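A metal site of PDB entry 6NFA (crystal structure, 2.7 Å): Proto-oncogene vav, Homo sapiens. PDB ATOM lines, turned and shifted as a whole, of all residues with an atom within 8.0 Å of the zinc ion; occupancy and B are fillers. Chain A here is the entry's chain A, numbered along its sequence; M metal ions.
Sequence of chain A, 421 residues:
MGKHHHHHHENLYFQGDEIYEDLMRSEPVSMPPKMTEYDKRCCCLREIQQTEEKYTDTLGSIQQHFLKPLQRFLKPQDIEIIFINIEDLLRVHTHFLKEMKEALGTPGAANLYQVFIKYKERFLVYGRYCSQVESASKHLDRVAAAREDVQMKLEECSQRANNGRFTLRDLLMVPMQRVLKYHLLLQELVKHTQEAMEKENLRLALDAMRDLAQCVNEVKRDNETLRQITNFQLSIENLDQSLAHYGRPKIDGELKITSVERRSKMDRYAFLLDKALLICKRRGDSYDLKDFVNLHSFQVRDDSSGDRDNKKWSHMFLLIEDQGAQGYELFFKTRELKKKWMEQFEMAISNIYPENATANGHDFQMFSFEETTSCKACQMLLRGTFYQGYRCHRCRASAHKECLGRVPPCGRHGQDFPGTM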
ATOM      1  N   SER A 374     -17.006 -25.161  20.841  1.00  0.00           N
ATOM      2  CA  SER A 374     -17.075 -24.199  19.757  1.00  0.00           C
ATOM      3  C   SER A 374     -18.499 -23.685  19.575  1.00  0.00           C
ATOM      4  O   SER A 374     -19.451 -24.387  19.885  1.00  0.00           O
ATOM      5  CB  SER A 374     -16.584 -24.834  18.455  1.00  0.00           C
ATOM      6  OG  SER A 374     -15.219 -25.161  18.560  1.00  0.00           O
ATOM      7  N   CYS A 375     -18.631 -22.472  19.044  1.00  0.00           N
ATOM      8  CA  CYS A 375     -19.904 -21.857  18.745  1.00  0.00           C
ATOM      9  C   CYS A 375     -20.496 -22.448  17.432  1.00  0.00           C
ATOM     10  O   CYS A 375     -19.873 -22.356  16.378  1.00  0.00           O
ATOM     11  CB  CYS A 375     -19.726 -20.346  18.631  1.00  0.00           C
ATOM     12  SG  CYS A 375     -21.183 -19.457  18.016  1.00  0.00           S
ATOM     13  N   LYS A 376     -21.725 -22.982  17.494  1.00  0.00           N
ATOM     14  CA  LYS A 376     -22.457 -23.543  16.342  1.00  0.00           C
ATOM     15  C   LYS A 376     -22.629 -22.539  15.146  1.00  0.00           C
ATOM     16  O   LYS A 376     -22.824 -22.986  14.016  1.00  0.00           O
ATOM     17  CB  LYS A 376     -23.832 -24.061  16.795  1.00  0.00           C
ATOM     18  CG  LYS A 376     -24.409 -25.158  15.915  1.00  0.00           C
ATOM     19  CD  LYS A 376     -23.821 -26.528  16.220  1.00  0.00           C
ATOM     20  CE  LYS A 376     -24.205 -27.524  15.165  1.00  0.00           C
ATOM     21  NZ  LYS A 376     -23.655 -28.876  15.462  1.00  0.00           N
ATOM     22  N   ALA A 377     -22.529 -21.220  15.388  1.00  0.00           N
ATOM     23  CA  ALA A 377     -22.676 -20.204  14.340  1.00  0.00           C
ATOM     24  C   ALA A 377     -21.337 -19.747  13.680  1.00  0.00           C
ATOM     25  O   ALA A 377     -21.220 -19.814  12.450  1.00  0.00           O
ATOM     26  CB  ALA A 377     -23.458 -19.021  14.862  1.00  0.00           C
ATOM     27  N   CYS A 378     -20.355 -19.276  14.481  1.00  0.00           N
ATOM     28  CA  CYS A 378     -19.065 -18.774  13.976  1.00  0.00           C
ATOM     29  C   CYS A 378     -17.946 -19.820  13.981  1.00  0.00           C
ATOM     30  O   CYS A 378     -16.882 -19.578  13.419  1.00  0.00           O
ATOM     31  CB  CYS A 378     -18.649 -17.503  14.703  1.00  0.00           C
ATOM     32  SG  CYS A 378     -18.282 -17.751  16.463  1.00  0.00           S
ATOM     33  N   GLN A 379     -18.179 -20.970  14.649  1.00  0.00           N
ATOM     34  CA  GLN A 379     -17.242 -22.109  14.788  1.00  0.00           C
ATOM     35  C   GLN A 379     -15.983 -21.755  15.639  1.00  0.00           C
ATOM     36  O   GLN A 379     -15.043 -22.559  15.737  1.00  0.00           O
ATOM     37  CB  GLN A 379     -16.881 -22.765  13.426  1.00  0.00           C
ATOM     38  CG  GLN A 379     -18.074 -23.169  12.544  1.00  0.00           C
ATOM     39  CD  GLN A 379     -19.034 -24.191  13.124  1.00  0.00           C
ATOM     40  OE1 GLN A 379     -18.700 -25.026  13.991  1.00  0.00           O
ATOM     41  NE2 GLN A 379     -20.262 -24.199  12.619  1.00  0.00           N
ATOM     42  N   MET A 380     -16.005 -20.608  16.324  1.00  0.00           N
ATOM     43  CA  MET A 380     -14.949 -20.177  17.241  1.00  0.00           C
ATOM     44  C   MET A 380     -15.213 -20.648  18.681  1.00  0.00           C
ATOM     45  O   MET A 380     -16.360 -20.854  19.068  1.00  0.00           O
ATOM     46  CB  MET A 380     -14.738 -18.657  17.178  1.00  0.00           C
ATOM     47  CG  MET A 380     -14.065 -18.218  15.893  1.00  0.00           C
ATOM     48  SD  MET A 380     -13.706 -16.456  15.851  1.00  0.00           S
ATOM     49  CE  MET A 380     -12.202 -16.380  16.859  1.00  0.00           C
ATOM     50  N   LEU A 381     -14.145 -20.771  19.463  1.00  0.00           N
ATOM     51  CA  LEU A 381     -14.127 -21.212  20.872  1.00  0.00           C
ATOM     52  C   LEU A 381     -14.960 -20.337  21.799  1.00  0.00           C
ATOM     53  O   LEU A 381     -14.926 -19.098  21.682  1.00  0.00           O
ATOM     54  CB  LEU A 381     -12.649 -21.197  21.367  1.00  0.00           C
ATOM     55  CG  LEU A 381     -12.358 -21.504  22.843  1.00  0.00           C
ATOM     56  CD1 LEU A 381     -12.440 -23.007  23.140  1.00  0.00           C
ATOM     57  CD2 LEU A 381     -11.032 -20.880  23.302  1.00  0.00           C
ATOM     58  N   LEU A 382     -15.667 -20.973  22.753  1.00  0.00           N
ATOM     59  CA  LEU A 382     -16.389 -20.292  23.830  1.00  0.00           C
ATOM     60  C   LEU A 382     -15.309 -20.145  24.923  1.00  0.00           C
ATOM     61  O   LEU A 382     -14.950 -21.106  25.597  1.00  0.00           O
ATOM     62  CB  LEU A 382     -17.585 -21.142  24.291  1.00  0.00           C
ATOM     63  CG  LEU A 382     -18.835 -21.038  23.400  1.00  0.00           C
ATOM     64  CD1 LEU A 382     -19.675 -22.262  23.517  1.00  0.00           C
ATOM     65  CD2 LEU A 382     -19.689 -19.872  23.803  1.00  0.00           C
ATOM     66  N   SER A 398     -24.413 -25.036  21.148  1.00  0.00           N
ATOM     67  CA  SER A 398     -23.667 -24.062  21.961  1.00  0.00           C
ATOM     68  C   SER A 398     -23.439 -22.824  21.127  1.00  0.00           C
ATOM     69  O   SER A 398     -23.271 -22.962  19.925  1.00  0.00           O
ATOM     70  CB  SER A 398     -22.314 -24.633  22.354  1.00  0.00           C
ATOM     71  OG  SER A 398     -22.398 -25.996  22.714  1.00  0.00           O
ATOM     72  N   ALA A 399     -23.391 -21.625  21.738  1.00  0.00           N
ATOM     73  CA  ALA A 399     -23.122 -20.389  20.982  1.00  0.00           C
ATOM     74  C   ALA A 399     -22.727 -19.197  21.849  1.00  0.00           C
ATOM     75  O   ALA A 399     -22.991 -19.201  23.043  1.00  0.00           O
ATOM     76  CB  ALA A 399     -24.334 -20.002  20.122  1.00  0.00           C
ATOM     77  N   HIS A 400     -22.136 -18.164  21.251  1.00  0.00           N
ATOM     78  CA  HIS A 400     -21.801 -16.941  21.945  1.00  0.00           C
ATOM     79  C   HIS A 400     -23.057 -16.101  22.087  1.00  0.00           C
ATOM     80  O   HIS A 400     -24.018 -16.291  21.316  1.00  0.00           O
ATOM     81  CB  HIS A 400     -20.804 -16.129  21.119  1.00  0.00           C
ATOM     82  CG  HIS A 400     -19.464 -16.770  20.980  1.00  0.00           C
ATOM     83  ND1 HIS A 400     -18.998 -17.182  19.749  1.00  0.00           N
ATOM     84  CD2 HIS A 400     -18.517 -17.010  21.908  1.00  0.00           C
ATOM     85  CE1 HIS A 400     -17.782 -17.667  19.968  1.00  0.00           C
ATOM     86  NE2 HIS A 400     -17.458 -17.594  21.260  1.00  0.00           N
ATOM     87  N   LYS A 401     -23.040 -15.138  23.048  1.00  0.00           N
ATOM     88  CA  LYS A 401     -24.176 -14.242  23.290  1.00  0.00           C
ATOM     89  C   LYS A 401     -24.637 -13.513  22.001  1.00  0.00           C
ATOM     90  O   LYS A 401     -25.834 -13.423  21.734  1.00  0.00           O
ATOM     91  CB  LYS A 401     -23.884 -13.225  24.436  1.00  0.00           C
ATOM     92  CG  LYS A 401     -25.161 -12.520  24.939  1.00  0.00           C
ATOM     93  CD  LYS A 401     -24.973 -11.542  26.063  1.00  0.00           C
ATOM     94  CE  LYS A 401     -26.287 -10.854  26.397  1.00  0.00           C
ATOM     95  NZ  LYS A 401     -26.080  -9.540  27.052  1.00  0.00           N
ATOM     96  N   GLU A 402     -23.680 -13.018  21.209  1.00  0.00           N
ATOM     97  CA  GLU A 402     -23.887 -12.232  19.990  1.00  0.00           C
ATOM     98  C   GLU A 402     -24.087 -13.057  18.699  1.00  0.00           C
ATOM     99  O   GLU A 402     -24.206 -12.461  17.628  1.00  0.00           O
ATOM    100  CB  GLU A 402     -22.709 -11.221  19.826  1.00  0.00           C
ATOM    101  CG  GLU A 402     -21.316 -11.826  19.647  1.00  0.00           C
ATOM    102  CD  GLU A 402     -20.498 -12.300  20.845  1.00  0.00           C
ATOM    103  OE1 GLU A 402     -21.047 -12.389  21.977  1.00  0.00           O
ATOM    104  OE2 GLU A 402     -19.306 -12.615  20.643  1.00  0.00           O
ATOM    105  N   CYS A 403     -24.147 -14.403  18.793  1.00  0.00           N
ATOM    106  CA  CYS A 403     -24.277 -15.328  17.661  1.00  0.00           C
ATOM    107  C   CYS A 403     -25.617 -16.061  17.576  1.00  0.00           C
ATOM    108  O   CYS A 403     -25.866 -16.719  16.561  1.00  0.00           O
ATOM    109  CB  CYS A 403     -23.107 -16.324  17.666  1.00  0.00           C
ATOM    110  SG  CYS A 403     -21.496 -15.610  17.234  1.00  0.00           S
ATOM    111  N   LEU A 404     -26.458 -16.010  18.642  1.00  0.00           N
ATOM    112  CA  LEU A 404     -27.739 -16.725  18.780  1.00  0.00           C
ATOM    113  C   LEU A 404     -28.660 -16.697  17.522  1.00  0.00           C
ATOM    114  O   LEU A 404     -29.143 -17.746  17.111  1.00  0.00           O
ATOM    115  CB  LEU A 404     -28.539 -16.259  20.017  1.00  0.00           C
ATOM    116  CG  LEU A 404     -27.842 -16.282  21.395  1.00  0.00           C
ATOM    117  CD1 LEU A 404     -28.815 -15.943  22.487  1.00  0.00           C
ATOM    118  CD2 LEU A 404     -27.180 -17.641  21.693  1.00  0.00           C
ATOM    119  N   ARG A 406     -27.804 -16.324  14.462  1.00  0.00           N
ATOM    120  CA  ARG A 406     -27.085 -16.895  13.339  1.00  0.00           C
ATOM    121  C   ARG A 406     -27.007 -18.402  13.422  1.00  0.00           C
ATOM    122  O   ARG A 406     -26.647 -19.039  12.428  1.00  0.00           O
ATOM    123  CB  ARG A 406     -25.675 -16.276  13.228  1.00  0.00           C
ATOM    124  CG  ARG A 406     -25.639 -14.774  12.861  1.00  0.00           C
ATOM    125  CD  ARG A 406     -26.728 -14.342  11.887  1.00  0.00           C
ATOM    126  NE  ARG A 406     -26.639 -15.066  10.615  1.00  0.00           N
ATOM    127  CZ  ARG A 406     -27.691 -15.454   9.901  1.00  0.00           C
ATOM    128  NH1 ARG A 406     -28.929 -15.208  10.327  1.00  0.00           N
ATOM    129  NH2 ARG A 406     -27.520 -16.103   8.758  1.00  0.00           N
ATOM    130  N   VAL A 407     -27.328 -18.982  14.589  1.00  0.00           N
ATOM    131  CA  VAL A 407     -27.274 -20.440  14.744  1.00  0.00           C
ATOM    132  C   VAL A 407     -28.309 -21.153  13.799  1.00  0.00           C
ATOM    133  O   VAL A 407     -29.352 -20.563  13.493  1.00  0.00           O
ATOM    134  CB  VAL A 407     -27.347 -20.947  16.208  1.00  0.00           C
ATOM    135  CG1 VAL A 407     -27.411 -22.479  16.284  1.00  0.00           C
ATOM    136  CG2 VAL A 407     -26.190 -20.432  17.019  1.00  0.00           C
HETATM  137 ZN    ZN M   1     -20.100 -17.352  17.867  1.00  0.00          ZN
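The backbone carbonyl oxygen (O) of Leu 381 is in hydrogen-bond range of a ring nitrogen (NE2) of His 400, at 3.0 Å. SG of Cys 378 sits close to N of Met 380, 3.7 Å away. The backbone NH of Cys 375 lies within hydrogen-bond range of the backbone carbonyl oxygen of Met 380 (2.8 Å). The side-chain sulfur (SG) of Cys 375 sits close to the backbone NH (N) of Ala 377 (3.4 Å).
The zinc ion is bound by a ring nitrogen (ND1) of His 400 (2.2 Å), the side-chain sulfur (SG) of Cys 403 (2.3 Å), the side-chain sulfur (SG) of Cys 378 (2.3 Å) and the side-chain sulfur (SG) of Cys 375 (2.4 Å).
Within 4 Å of the zinc ion: Cys 375, Cys 378, His 400 and Cys 403.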
